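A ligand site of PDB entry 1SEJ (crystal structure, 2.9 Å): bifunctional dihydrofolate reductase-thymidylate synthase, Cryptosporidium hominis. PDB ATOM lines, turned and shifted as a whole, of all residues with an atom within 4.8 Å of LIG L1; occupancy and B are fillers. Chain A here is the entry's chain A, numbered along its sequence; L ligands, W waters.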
ATOM      1  N   VAL A   9     -11.686 -29.909  19.128  1.00  0.00           N
ATOM      2  CA  VAL A   9     -12.490 -29.652  20.301  1.00  0.00           C
ATOM      3  C   VAL A   9     -12.663 -28.145  20.330  1.00  0.00           C
ATOM      4  O   VAL A   9     -11.674 -27.397  20.353  1.00  0.00           O
ATOM      5  CB  VAL A   9     -11.788 -30.081  21.571  1.00  0.00           C
ATOM      6  CG1 VAL A   9     -12.742 -29.990  22.741  1.00  0.00           C
ATOM      7  CG2 VAL A   9     -11.291 -31.487  21.415  1.00  0.00           C
ATOM      8  N   VAL A  10     -13.907 -27.676  20.318  1.00  0.00           N
ATOM      9  CA  VAL A  10     -14.177 -26.256  20.321  1.00  0.00           C
ATOM     10  C   VAL A  10     -15.566 -25.938  20.839  1.00  0.00           C
ATOM     11  O   VAL A  10     -16.474 -26.775  20.803  1.00  0.00           O
ATOM     12  CB  VAL A  10     -14.029 -25.685  18.880  1.00  0.00           C
ATOM     13  CG1 VAL A  10     -15.047 -26.354  17.968  1.00  0.00           C
ATOM     14  CG2 VAL A  10     -14.209 -24.169  18.880  1.00  0.00           C
ATOM     15  N   ALA A  11     -15.730 -24.715  21.335  1.00  0.00           N
ATOM     16  CA  ALA A  11     -17.011 -24.238  21.824  1.00  0.00           C
ATOM     17  C   ALA A  11     -17.228 -22.908  21.102  1.00  0.00           C
ATOM     18  O   ALA A  11     -16.405 -21.999  21.189  1.00  0.00           O
ATOM     19  CB  ALA A  11     -16.953 -24.045  23.308  1.00  0.00           C
ATOM     20  N   ILE A  19     -15.852 -17.740  19.090  1.00  0.00           N
ATOM     21  CA  ILE A  19     -15.138 -18.555  20.061  1.00  0.00           C
ATOM     22  C   ILE A  19     -14.191 -17.776  20.946  1.00  0.00           C
ATOM     23  O   ILE A  19     -13.674 -18.301  21.926  1.00  0.00           O
ATOM     24  CB  ILE A  19     -14.304 -19.649  19.379  1.00  0.00           C
ATOM     25  CG1 ILE A  19     -13.232 -19.014  18.508  1.00  0.00           C
ATOM     26  CG2 ILE A  19     -15.194 -20.538  18.530  1.00  0.00           C
ATOM     27  CD1 ILE A  19     -12.122 -19.955  18.172  1.00  0.00           C
ATOM     28  N   GLY A  20     -13.947 -16.518  20.604  1.00  0.00           N
ATOM     29  CA  GLY A  20     -13.040 -15.729  21.419  1.00  0.00           C
ATOM     30  C   GLY A  20     -13.227 -14.230  21.337  1.00  0.00           C
ATOM     31  O   GLY A  20     -13.795 -13.706  20.375  1.00  0.00           O
ATOM     32  N   ILE A  21     -12.752 -13.539  22.365  1.00  0.00           N
ATOM     33  CA  ILE A  21     -12.828 -12.098  22.454  1.00  0.00           C
ATOM     34  C   ILE A  21     -11.690 -11.600  23.341  1.00  0.00           C
ATOM     35  O   ILE A  21     -11.564 -12.028  24.495  1.00  0.00           O
ATOM     36  CB  ILE A  21     -14.200 -11.643  23.019  1.00  0.00           C
ATOM     37  CG1 ILE A  21     -14.217 -10.119  23.154  1.00  0.00           C
ATOM     38  CG2 ILE A  21     -14.483 -12.339  24.340  1.00  0.00           C
ATOM     39  CD1 ILE A  21     -14.037  -9.389  21.852  1.00  0.00           C
ATOM     40  N   GLY A  23      -8.550 -12.267  23.494  1.00  0.00           N
ATOM     41  CA  GLY A  23      -7.769 -13.349  24.074  1.00  0.00           C
ATOM     42  C   GLY A  23      -8.415 -14.179  25.167  1.00  0.00           C
ATOM     43  O   GLY A  23      -7.721 -14.803  25.957  1.00  0.00           O
ATOM     44  N   GLN A  24      -9.735 -14.175  25.231  1.00  0.00           N
ATOM     45  CA  GLN A  24     -10.433 -14.930  26.247  1.00  0.00           C
ATOM     46  C   GLN A  24     -11.659 -15.566  25.621  1.00  0.00           C
ATOM     47  O   GLN A  24     -12.014 -15.239  24.496  1.00  0.00           O
ATOM     48  CB  GLN A  24     -10.905 -13.999  27.371  1.00  0.00           C
ATOM     49  CG  GLN A  24      -9.866 -13.194  28.080  1.00  0.00           C
ATOM     50  CD  GLN A  24     -10.495 -12.046  28.850  1.00  0.00           C
ATOM     51  OE1 GLN A  24      -9.859 -11.416  29.700  1.00  0.00           O
ATOM     52  NE2 GLN A  24     -11.762 -11.751  28.549  1.00  0.00           N
ATOM     53  N   LEU A  25     -12.306 -16.463  26.351  1.00  0.00           N
ATOM     54  CA  LEU A  25     -13.524 -17.071  25.857  1.00  0.00           C
ATOM     55  C   LEU A  25     -14.562 -15.982  26.052  1.00  0.00           C
ATOM     56  O   LEU A  25     -14.419 -15.139  26.918  1.00  0.00           O
ATOM     57  CB  LEU A  25     -13.888 -18.308  26.667  1.00  0.00           C
ATOM     58  CG  LEU A  25     -12.872 -19.442  26.560  1.00  0.00           C
ATOM     59  CD1 LEU A  25     -13.298 -20.589  27.433  1.00  0.00           C
ATOM     60  CD2 LEU A  25     -12.751 -19.889  25.129  1.00  0.00           C
ATOM     61  N   TRP A  27     -17.368 -16.235  27.345  1.00  0.00           N
ATOM     62  CA  TRP A  27     -18.292 -16.697  28.368  1.00  0.00           C
ATOM     63  C   TRP A  27     -17.528 -17.563  29.369  1.00  0.00           C
ATOM     64  O   TRP A  27     -16.388 -17.941  29.121  1.00  0.00           O
ATOM     65  CB  TRP A  27     -19.407 -17.525  27.726  1.00  0.00           C
ATOM     66  CG  TRP A  27     -18.862 -18.660  26.925  1.00  0.00           C
ATOM     67  CD1 TRP A  27     -18.219 -19.769  27.409  1.00  0.00           C
ATOM     68  CD2 TRP A  27     -18.809 -18.757  25.499  1.00  0.00           C
ATOM     69  NE1 TRP A  27     -17.749 -20.540  26.372  1.00  0.00           N
ATOM     70  CE2 TRP A  27     -18.095 -19.940  25.190  1.00  0.00           C
ATOM     71  CE3 TRP A  27     -19.281 -17.955  24.454  1.00  0.00           C
ATOM     72  CZ2 TRP A  27     -17.847 -20.331  23.866  1.00  0.00           C
ATOM     73  CZ3 TRP A  27     -19.028 -18.354  23.139  1.00  0.00           C
ATOM     74  CH2 TRP A  27     -18.320 -19.531  22.860  1.00  0.00           C
ATOM     75  N   GLY A  55      -2.649 -22.926  18.646  1.00  0.00           N
ATOM     76  CA  GLY A  55      -1.903 -21.771  18.183  1.00  0.00           C
ATOM     77  C   GLY A  55      -1.203 -21.088  19.347  1.00  0.00           C
ATOM     78  O   GLY A  55      -1.562 -21.308  20.488  1.00  0.00           O
ATOM     79  N   ARG A  56      -0.211 -20.266  19.054  1.00  0.00           N
ATOM     80  CA  ARG A  56       0.520 -19.581  20.109  1.00  0.00           C
ATOM     81  C   ARG A  56      -0.378 -18.731  20.977  1.00  0.00           C
ATOM     82  O   ARG A  56      -0.256 -18.747  22.202  1.00  0.00           O
ATOM     83  CB  ARG A  56       1.606 -18.678  19.542  1.00  0.00           C
ATOM     84  CG  ARG A  56       2.522 -18.154  20.614  1.00  0.00           C
ATOM     85  CD  ARG A  56       3.070 -16.814  20.254  1.00  0.00           C
ATOM     86  NE  ARG A  56       2.146 -15.755  20.592  1.00  0.00           N
ATOM     87  CZ  ARG A  56       1.806 -14.782  19.769  1.00  0.00           C
ATOM     88  NH1 ARG A  56       2.308 -14.740  18.542  1.00  0.00           N
ATOM     89  NH2 ARG A  56       0.981 -13.825  20.173  1.00  0.00           N
ATOM     90  N   LYS A  57      -1.264 -17.969  20.350  1.00  0.00           N
ATOM     91  CA  LYS A  57      -2.159 -17.114  21.098  1.00  0.00           C
ATOM     92  C   LYS A  57      -2.996 -17.899  22.088  1.00  0.00           C
ATOM     93  O   LYS A  57      -3.205 -17.460  23.216  1.00  0.00           O
ATOM     94  CB  LYS A  57      -3.052 -16.298  20.152  1.00  0.00           C
ATOM     95  CG  LYS A  57      -2.282 -15.291  19.321  1.00  0.00           C
ATOM     96  CD  LYS A  57      -3.199 -14.287  18.654  1.00  0.00           C
ATOM     97  CE  LYS A  57      -2.406 -13.335  17.751  1.00  0.00           C
ATOM     98  NZ  LYS A  57      -3.263 -12.298  17.117  1.00  0.00           N
ATOM     99  N   THR A  58      -3.463 -19.081  21.677  1.00  0.00           N
ATOM    100  CA  THR A  58      -4.254 -19.905  22.596  1.00  0.00           C
ATOM    101  C   THR A  58      -3.355 -20.367  23.740  1.00  0.00           C
ATOM    102  O   THR A  58      -3.788 -20.443  24.887  1.00  0.00           O
ATOM    103  CB  THR A  58      -4.869 -21.116  21.889  1.00  0.00           C
ATOM    104  OG1 THR A  58      -5.867 -20.659  20.973  1.00  0.00           O
ATOM    105  CG2 THR A  58      -5.519 -22.048  22.887  1.00  0.00           C
ATOM    106  N   SER A  61      -3.353 -17.960  26.162  1.00  0.00           N
ATOM    107  CA  SER A  61      -4.616 -18.006  26.896  1.00  0.00           C
ATOM    108  C   SER A  61      -4.525 -18.916  28.096  1.00  0.00           C
ATOM    109  O   SER A  61      -5.078 -18.614  29.147  1.00  0.00           O
ATOM    110  CB  SER A  61      -5.724 -18.543  26.008  1.00  0.00           C
ATOM    111  OG  SER A  61      -5.807 -17.792  24.821  1.00  0.00           O
ATOM    112  N   ILE A  75       1.950 -24.251  17.926  1.00  0.00           N
ATOM    113  CA  ILE A  75       2.352 -23.903  16.572  1.00  0.00           C
ATOM    114  C   ILE A  75       2.711 -22.416  16.605  1.00  0.00           C
ATOM    115  O   ILE A  75       1.854 -21.567  16.833  1.00  0.00           O
ATOM    116  CB  ILE A  75       1.223 -24.138  15.548  1.00  0.00           C
ATOM    117  CG1 ILE A  75       1.167 -25.608  15.134  1.00  0.00           C
ATOM    118  CG2 ILE A  75       1.485 -23.321  14.293  1.00  0.00           C
ATOM    119  CD1 ILE A  75       0.927 -26.557  16.243  1.00  0.00           C
ATOM    120  N   SER A  76       3.990 -22.108  16.394  1.00  0.00           N
ATOM    121  CA  SER A  76       4.429 -20.721  16.374  1.00  0.00           C
ATOM    122  C   SER A  76       5.634 -20.602  15.462  1.00  0.00           C
ATOM    123  O   SER A  76       6.397 -21.550  15.306  1.00  0.00           O
ATOM    124  CB  SER A  76       4.819 -20.246  17.770  1.00  0.00           C
ATOM    125  OG  SER A  76       5.253 -18.901  17.738  1.00  0.00           O
ATOM    126  N   SER A  77       5.807 -19.429  14.863  1.00  0.00           N
ATOM    127  CA  SER A  77       6.940 -19.201  13.984  1.00  0.00           C
ATOM    128  C   SER A  77       8.089 -18.630  14.794  1.00  0.00           C
ATOM    129  O   SER A  77       9.244 -18.752  14.409  1.00  0.00           O
ATOM    130  CB  SER A  77       6.549 -18.222  12.889  1.00  0.00           C
ATOM    131  OG  SER A  77       6.319 -16.950  13.436  1.00  0.00           O
ATOM    132  N   SER A  78       7.762 -18.004  15.928  1.00  0.00           N
ATOM    133  CA  SER A  78       8.766 -17.394  16.786  1.00  0.00           C
ATOM    134  C   SER A  78       9.158 -18.237  17.988  1.00  0.00           C
ATOM    135  O   SER A  78      10.323 -18.569  18.164  1.00  0.00           O
ATOM    136  CB  SER A  78       8.270 -16.035  17.290  1.00  0.00           C
ATOM    137  OG  SER A  78       7.129 -16.167  18.134  1.00  0.00           O
ATOM    138  N   ARG A  92       6.990 -25.307  13.876  1.00  0.00           N
ATOM    139  CA  ARG A  92       6.895 -24.156  12.988  1.00  0.00           C
ATOM    140  C   ARG A  92       5.666 -24.042  12.099  1.00  0.00           C
ATOM    141  O   ARG A  92       5.269 -22.949  11.711  1.00  0.00           O
ATOM    142  CB  ARG A  92       8.156 -24.032  12.138  1.00  0.00           C
ATOM    143  CG  ARG A  92       9.403 -23.701  12.929  1.00  0.00           C
ATOM    144  CD  ARG A  92       9.177 -22.459  13.775  1.00  0.00           C
ATOM    145  NE  ARG A  92      10.292 -22.245  14.678  1.00  0.00           N
ATOM    146  CZ  ARG A  92      10.216 -21.552  15.821  1.00  0.00           C
ATOM    147  NH1 ARG A  92       9.065 -21.022  16.196  1.00  0.00           N
ATOM    148  NH2 ARG A  92      11.288 -21.417  16.578  1.00  0.00           N
ATOM    149  N   ASN A  93       5.075 -25.181  11.736  1.00  0.00           N
ATOM    150  CA  ASN A  93       3.874 -25.174  10.903  1.00  0.00           C
ATOM    151  C   ASN A  93       2.999 -26.328  11.383  1.00  0.00           C
ATOM    152  O   ASN A  93       3.497 -27.275  12.001  1.00  0.00           O
ATOM    153  CB  ASN A  93       4.212 -25.339   9.401  1.00  0.00           C
ATOM    154  CG  ASN A  93       4.481 -26.774   9.008  1.00  0.00           C
ATOM    155  OD1 ASN A  93       5.450 -27.367   9.456  1.00  0.00           O
ATOM    156  ND2 ASN A  93       3.618 -27.339   8.175  1.00  0.00           N
ATOM    157  N   CYS A 113      -6.751 -28.188  19.418  1.00  0.00           N
ATOM    158  CA  CYS A 113      -7.349 -27.365  20.453  1.00  0.00           C
ATOM    159  C   CYS A 113      -7.542 -25.879  20.240  1.00  0.00           C
ATOM    160  O   CYS A 113      -7.724 -25.150  21.213  1.00  0.00           O
ATOM    161  CB  CYS A 113      -6.607 -27.587  21.755  1.00  0.00           C
ATOM    162  SG  CYS A 113      -6.775 -29.272  22.299  1.00  0.00           S
ATOM    163  N   GLY A 114      -7.474 -25.389  19.024  1.00  0.00           N
ATOM    164  CA  GLY A 114      -7.745 -23.992  18.925  1.00  0.00           C
ATOM    165  C   GLY A 114      -6.847 -22.955  18.320  1.00  0.00           C
ATOM    166  O   GLY A 114      -5.628 -23.087  18.206  1.00  0.00           O
ATOM    167  N   GLY A 115      -7.547 -21.870  18.013  1.00  0.00           N
ATOM    168  CA  GLY A 115      -6.996 -20.709  17.374  1.00  0.00           C
ATOM    169  C   GLY A 115      -7.778 -20.731  16.079  1.00  0.00           C
ATOM    170  O   GLY A 115      -7.731 -21.736  15.370  1.00  0.00           O
ATOM    171  N   GLU A 116      -8.518 -19.677  15.790  1.00  0.00           N
ATOM    172  CA  GLU A 116      -9.266 -19.651  14.549  1.00  0.00           C
ATOM    173  C   GLU A 116      -8.316 -20.087  13.442  1.00  0.00           C
ATOM    174  O   GLU A 116      -8.660 -20.935  12.630  1.00  0.00           O
ATOM    175  CB  GLU A 116      -9.783 -18.247  14.263  1.00  0.00           C
ATOM    176  CG  GLU A 116     -10.422 -18.121  12.900  1.00  0.00           C
ATOM    177  CD  GLU A 116     -11.153 -16.811  12.734  1.00  0.00           C
ATOM    178  OE1 GLU A 116     -11.623 -16.548  11.612  1.00  0.00           O
ATOM    179  OE2 GLU A 116     -11.245 -16.051  13.730  1.00  0.00           O
ATOM    180  N   SER A 117      -7.110 -19.538  13.452  1.00  0.00           N
ATOM    181  CA  SER A 117      -6.119 -19.870  12.431  1.00  0.00           C
ATOM    182  C   SER A 117      -5.828 -21.361  12.356  1.00  0.00           C
ATOM    183  O   SER A 117      -5.878 -21.962  11.284  1.00  0.00           O
ATOM    184  CB  SER A 117      -4.819 -19.104  12.705  1.00  0.00           C
ATOM    185  OG  SER A 117      -4.198 -19.568  13.881  1.00  0.00           O
ATOM    186  N   ILE A 118      -5.519 -21.974  13.486  1.00  0.00           N
ATOM    187  CA  ILE A 118      -5.213 -23.393  13.505  1.00  0.00           C
ATOM    188  C   ILE A 118      -6.424 -24.252  13.149  1.00  0.00           C
ATOM    189  O   ILE A 118      -6.284 -25.301  12.511  1.00  0.00           O
ATOM    190  CB  ILE A 118      -4.685 -23.820  14.881  1.00  0.00           C
ATOM    191  CG1 ILE A 118      -3.468 -22.970  15.256  1.00  0.00           C
ATOM    192  CG2 ILE A 118      -4.315 -25.302  14.858  1.00  0.00           C
ATOM    193  CD1 ILE A 118      -2.315 -23.091  14.301  1.00  0.00           C
ATOM    194  N   TYR A 119      -7.621 -23.847  13.557  1.00  0.00           N
ATOM    195  CA  TYR A 119      -8.805 -24.610  13.217  1.00  0.00           C
ATOM    196  C   TYR A 119      -8.965 -24.603  11.701  1.00  0.00           C
ATOM    197  O   TYR A 119      -8.967 -25.646  11.048  1.00  0.00           O
ATOM    198  CB  TYR A 119     -10.064 -23.993  13.834  1.00  0.00           C
ATOM    199  CG  TYR A 119     -10.267 -24.279  15.296  1.00  0.00           C
ATOM    200  CD1 TYR A 119     -10.184 -25.580  15.786  1.00  0.00           C
ATOM    201  CD2 TYR A 119     -10.602 -23.262  16.188  1.00  0.00           C
ATOM    202  CE1 TYR A 119     -10.441 -25.852  17.118  1.00  0.00           C
ATOM    203  CE2 TYR A 119     -10.864 -23.526  17.510  1.00  0.00           C
ATOM    204  CZ  TYR A 119     -10.781 -24.825  17.980  1.00  0.00           C
ATOM    205  OH  TYR A 119     -11.064 -25.093  19.291  1.00  0.00           O
ATOM    206  N   ASP A 121      -6.962 -23.954   9.353  1.00  0.00           N
ATOM    207  CA  ASP A 121      -5.907 -24.675   8.636  1.00  0.00           C
ATOM    208  C   ASP A 121      -6.056 -26.169   8.769  1.00  0.00           C
ATOM    209  O   ASP A 121      -5.861 -26.901   7.817  1.00  0.00           O
ATOM    210  CB  ASP A 121      -4.525 -24.282   9.154  1.00  0.00           C
ATOM    211  CG  ASP A 121      -3.998 -23.038   8.488  1.00  0.00           C
ATOM    212  OD1 ASP A 121      -2.881 -22.616   8.850  1.00  0.00           O
ATOM    213  OD2 ASP A 121      -4.698 -22.479   7.605  1.00  0.00           O
ATOM    214  N   ASP A 144     -14.171 -11.680  18.361  1.00  0.00           N
ATOM    215  CA  ASP A 144     -13.098 -11.307  17.447  1.00  0.00           C
ATOM    216  C   ASP A 144     -12.421 -12.550  16.864  1.00  0.00           C
ATOM    217  O   ASP A 144     -11.550 -12.462  16.021  1.00  0.00           O
ATOM    218  CB  ASP A 144     -12.064 -10.391  18.111  1.00  0.00           C
ATOM    219  CG  ASP A 144     -11.386 -11.014  19.301  1.00  0.00           C
ATOM    220  OD1 ASP A 144     -11.199 -12.258  19.286  1.00  0.00           O
ATOM    221  OD2 ASP A 144     -11.020 -10.253  20.230  1.00  0.00           O
ATOM    222  N   THR A 145     -12.855 -13.717  17.326  1.00  0.00           N
ATOM    223  CA  THR A 145     -12.311 -14.976  16.838  1.00  0.00           C
ATOM    224  C   THR A 145     -13.464 -15.932  16.549  1.00  0.00           C
ATOM    225  O   THR A 145     -14.413 -16.027  17.310  1.00  0.00           O
ATOM    226  CB  THR A 145     -11.350 -15.591  17.866  1.00  0.00           C
ATOM    227  OG1 THR A 145     -10.346 -14.625  18.201  1.00  0.00           O
ATOM    228  CG2 THR A 145     -10.686 -16.818  17.293  1.00  0.00           C
HETATM  229  P1  LIG L   1      -4.564 -18.868  17.641  1.00  0.00           P
HETATM  230  O1  LIG L   1      -4.652 -19.531  16.344  1.00  0.00           O
HETATM  231  O2  LIG L   1      -4.468 -19.563  18.942  1.00  0.00           O
HETATM  232  O3  LIG L   1      -3.015 -18.444  17.544  1.00  0.00           O
HETATM  233  C1  LIG L   1      -2.476 -17.782  16.389  1.00  0.00           C
HETATM  234  C2  LIG L   1      -0.961 -17.927  16.354  1.00  0.00           C
HETATM  235  O4  LIG L   1      -0.525 -19.315  16.147  1.00  0.00           O
HETATM  236  C3  LIG L   1      -0.286 -17.150  15.258  1.00  0.00           C
HETATM  237  O5  LIG L   1      -0.075 -15.800  15.681  1.00  0.00           O
HETATM  238  C4  LIG L   1       1.031 -17.838  15.161  1.00  0.00           C
HETATM  239  O6  LIG L   1       1.854 -17.474  16.253  1.00  0.00           O
HETATM  240  C5  LIG L   1       0.678 -19.312  15.279  1.00  0.00           C
HETATM  241  N1  LIG L   1       0.291 -19.812  13.932  1.00  0.00           N
HETATM  242  C6  LIG L   1      -0.938 -19.860  13.405  1.00  0.00           C
HETATM  243  N2  LIG L   1      -0.876 -20.345  12.161  1.00  0.00           N
HETATM  244  C7  LIG L   1       0.401 -20.605  11.903  1.00  0.00           C
HETATM  245  C8  LIG L   1       1.056 -21.117  10.794  1.00  0.00           C
HETATM  246  N3  LIG L   1       0.364 -21.456   9.707  1.00  0.00           N
HETATM  247  N4  LIG L   1       2.403 -21.280  10.833  1.00  0.00           N
HETATM  248  C9  LIG L   1       3.101 -20.950  11.930  1.00  0.00           C
HETATM  249  N5  LIG L   1       2.481 -20.448  13.009  1.00  0.00           N
HETATM  250  C10 LIG L   1       1.134 -20.273  13.011  1.00  0.00           C
HETATM  251  O7  LIG L   1      -5.096 -17.312  17.743  1.00  0.00           O
HETATM  252  P2  LIG L   1      -6.684 -16.939  17.567  1.00  0.00           P
HETATM  253  O8  LIG L   1      -6.878 -17.543  16.230  1.00  0.00           O
HETATM  254  O9  LIG L   1      -6.602 -15.507  17.830  1.00  0.00           O
HETATM  255  O10 LIG L   1      -7.102 -17.914  18.810  1.00  0.00           O
HETATM  256  C11 LIG L   1      -7.126 -17.440  20.175  1.00  0.00           C
HETATM  257  C12 LIG L   1      -8.520 -16.869  20.495  1.00  0.00           C
HETATM  258  O11 LIG L   1      -9.492 -17.952  20.285  1.00  0.00           O
HETATM  259  C13 LIG L   1      -8.649 -16.530  21.980  1.00  0.00           C
HETATM  260  O12 LIG L   1      -9.634 -15.527  22.173  1.00  0.00           O
HETATM  261  C14 LIG L   1      -9.093 -17.798  22.617  1.00  0.00           C
HETATM  262  O13 LIG L   1      -9.830 -17.515  23.813  1.00  0.00           O
HETATM  263  C15 LIG L   1     -10.026 -18.386  21.581  1.00  0.00           C
HETATM  264  N6  LIG L   1     -10.191 -19.854  21.665  1.00  0.00           N
HETATM  265  C16 LIG L   1     -11.485 -20.388  21.844  1.00  0.00           C
HETATM  266  C17 LIG L   1     -11.660 -21.773  21.861  1.00  0.00           C
HETATM  267  C18 LIG L   1     -13.068 -22.369  22.004  1.00  0.00           C
HETATM  268  O14 LIG L   1     -13.254 -23.582  21.909  1.00  0.00           O
HETATM  269  N7  LIG L   1     -14.032 -21.476  22.221  1.00  0.00           N
HETATM  270  C19 LIG L   1     -10.556 -22.623  21.720  1.00  0.00           C
HETATM  271  C20 LIG L   1      -9.257 -22.098  21.561  1.00  0.00           C
HETATM  272  C21 LIG L   1      -9.068 -20.715  21.533  1.00  0.00           C
HETATM  273  P3  LIG L   1       3.299 -16.834  15.983  1.00  0.00           P
HETATM  274  O15 LIG L   1       3.944 -16.682  17.470  1.00  0.00           O
HETATM  275  O16 LIG L   1       4.110 -17.405  14.926  1.00  0.00           O
HETATM  276  O17 LIG L   1       2.903 -15.439  15.700  1.00  0.00           O
HETATM  277  C1  LG2 L   2     -13.351 -24.861  25.700  1.00  0.00           C
HETATM  278  O1  LG2 L   2     -13.510 -24.075  26.625  1.00  0.00           O
HETATM  279  N1  LG2 L   2     -14.422 -25.687  25.330  1.00  0.00           N
HETATM  280  C2  LG2 L   2     -14.280 -26.570  24.249  1.00  0.00           C
HETATM  281  C3  LG2 L   2     -15.432 -27.484  23.842  1.00  0.00           C
HETATM  282  N2  LG2 L   2     -13.114 -26.601  23.588  1.00  0.00           N
HETATM  283  C4  LG2 L   2     -12.078 -25.826  23.925  1.00  0.00           C
HETATM  284  C5  LG2 L   2     -10.907 -25.939  23.180  1.00  0.00           C
HETATM  285  C6  LG2 L   2      -9.717 -25.071  23.566  1.00  0.00           C
HETATM  286  C7  LG2 L   2      -9.855 -24.211  24.646  1.00  0.00           C
HETATM  287  C8  LG2 L   2      -8.746 -23.469  25.043  1.00  0.00           C
HETATM  288  C9  LG2 L   2      -8.811 -22.641  26.163  1.00  0.00           C
HETATM  289  C10 LG2 L   2     -10.006 -22.559  26.876  1.00  0.00           C
HETATM  290  C11 LG2 L   2     -11.109 -23.308  26.468  1.00  0.00           C
HETATM  291  C12 LG2 L   2     -11.053 -24.142  25.357  1.00  0.00           C
HETATM  292  C13 LG2 L   2     -12.154 -24.930  24.998  1.00  0.00           C
HETATM  293  C14 LG2 L   2     -10.109 -21.675  28.118  1.00  0.00           C
HETATM  294  N3  LG2 L   2      -8.852 -21.651  28.885  1.00  0.00           N
HETATM  295  C15 LG2 L   2      -8.430 -22.660  29.658  1.00  0.00           C
HETATM  296  C16 LG2 L   2      -9.159 -23.843  29.791  1.00  0.00           C
HETATM  297  C17 LG2 L   2      -8.703 -24.854  30.635  1.00  0.00           C
HETATM  298  C18 LG2 L   2      -7.526 -24.687  31.337  1.00  0.00           C
HETATM  299  C19 LG2 L   2      -6.777 -23.514  31.204  1.00  0.00           C
HETATM  300  C20 LG2 L   2      -7.241 -22.509  30.360  1.00  0.00           C
HETATM  301  C21 LG2 L   2      -9.221 -26.032  30.974  1.00  0.00           C
HETATM  302  C22 LG2 L   2      -7.393 -25.831  32.116  1.00  0.00           C
HETATM  303  O2  LG2 L   2      -6.503 -26.040  32.941  1.00  0.00           O
HETATM  304  N4  LG2 L   2      -8.440 -26.617  31.878  1.00  0.00           N
HETATM  305  C23 LG2 L   2      -8.721 -27.888  32.569  1.00  0.00           C
HETATM  306  C24 LG2 L   2      -8.023 -29.048  31.860  1.00  0.00           C
HETATM  307  O3  LG2 L   2      -7.741 -28.987  30.669  1.00  0.00           O
HETATM  308  O4  LG2 L   2      -7.757 -30.073  32.489  1.00  0.00           O
HETATM  309  C25 LG2 L   2     -10.227 -28.165  32.595  1.00  0.00           C
HETATM  310  C26 LG2 L   2     -10.993 -27.175  33.463  1.00  0.00           C
HETATM  311  C27 LG2 L   2     -11.127 -27.697  34.896  1.00  0.00           C
HETATM  312  O5  LG2 L   2     -10.123 -27.991  35.551  1.00  0.00           O
HETATM  313  O6  LG2 L   2     -12.243 -27.864  35.388  1.00  0.00           O
HETATM  314  O   HOH W   1      -7.188 -13.789  20.142  1.00  0.00           O
HETATM  315  O   HOH W   2      -9.513 -13.001  20.968  1.00  0.00           O
HETATM  316  O   HOH W   3      -8.797 -18.908  25.736  1.00  0.00           O
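The backbone carbonyl oxygen (O) of Ile 75 lies close to an oxygen (O4) of LIG L1 (3.3 Å). The backbone carbonyl oxygen (O) of Arg 92 lies close to a nitrogen (N4) of LIG L1 (3.4 Å). Residues that only touch LIG L1: Val 10, Gly 20, Ile 21, Gly 23, Leu 25, Gly 55, Ser 61, Cys 113, Gly 114, Gly 115, Ile 118, Tyr 119, Asp 121 and Thr 145. Hydrophobic or aromatic side chains that line LIG L1: Val 10, Ala 11, Ile 19, Leu 25, Ile 75 and Ile 118. The nearest printed residue that does not touch LIG L1 is Asn 93 (4.2 Å).
An oxygen (O14) of LIG L1 lies close to a nitrogen (N2) of LG2 L2 (3.5 Å).
Water W3 lies within hydrogen-bond range of O13 of LIG L1 (2.6 Å) and OG of Ser 61 (3.3 Å). Water W2 lies within hydrogen-bond range of OD1 of Asp 144 (2.5 Å), O12 of LIG L1 (2.8 Å), N of Gly 23 (2.8 Å) and OG1 of Thr 145 (3.3 Å).
N of Arg 56 lies within hydrogen-bond range of O of Ile 75. N of Thr 145 is in hydrogen-bond range of O of Gly 20, at 3.2 Å. O of Ser 76 is in hydrogen-bond range of NH1 of Arg 92 (2.9 Å). OG of Ser 61 lies close to O of Thr 58 (3.3 Å). NH1 of Arg 92 lies close to O of Ser 78 (3.4 Å). The backbone NH of Gly 55 is in hydrogen-bond range of the backbone carbonyl oxygen of Gly 114 (3.0 Å). The backbone carbonyl oxygen of Thr 145 lies within hydrogen-bond range of the backbone NH of Ile 19 (2.9 Å). The side-chain hydroxyl of Ser 76 lies within hydrogen-bond range of the backbone NH of Ser 78 (3.2 Å).
O of Ile 19 sits close to N7 of LIG L1 (3.2 Å). The side-chain hydroxyl (OG1) of Thr 58 lies within hydrogen-bond range of an oxygen (O2) of LIG L1 (2.7 Å). O of Gln 24 sits at hydrogen-bond distance from O13 of LIG L1 (3.2 Å). N of Ser 77 sits at hydrogen-bond distance from O16 of LIG L1 (2.6 Å). A nitrogen (N7) of LIG L1 is in hydrogen-bond range of the backbone carbonyl oxygen (O) of Ala 11, 2.6 Å away. The backbone NH of Ala 11 sits at hydrogen-bond distance from an oxygen (O14) of LIG L1 (2.8 Å). OG of Ser 117 sits at hydrogen-bond distance from O1 of LIG L1 (2.5 Å). OG of Ser 78 is in hydrogen-bond range of O15 of LIG L1, 3.3 Å away. The backbone NH (N) of Gln 24 sits at hydrogen-bond distance from an oxygen (O12) of LIG L1, 3.3 Å away. The guanidinium group (NH1) of Arg 56 lies within salt-bridge range of an oxygen (O15) of LIG L1. The backbone NH of Glu 116 lies within hydrogen-bond range of an oxygen (O8) of LIG L1 (2.7 Å). N of Lys 57 is in hydrogen-bond range of O3 of LIG L1, 3.3 Å away. An oxygen (O8) of LIG L1 lies within hydrogen-bond range of the backbone NH (N) of Ser 117, 3.4 Å away. O2 of LIG L1 sits at hydrogen-bond distance from N of Thr 58. The side-chain hydroxyl (OG) of Ser 77 sits at hydrogen-bond distance from an oxygen (O16) of LIG L1, 2.7 Å away. The side-chain hydroxyl (OG) of Ser 76 is in hydrogen-bond range of an oxygen (O15) of LIG L1 (2.6 Å). The backbone NH (N) of Arg 56 lies within hydrogen-bond range of an oxygen (O4) of LIG L1.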
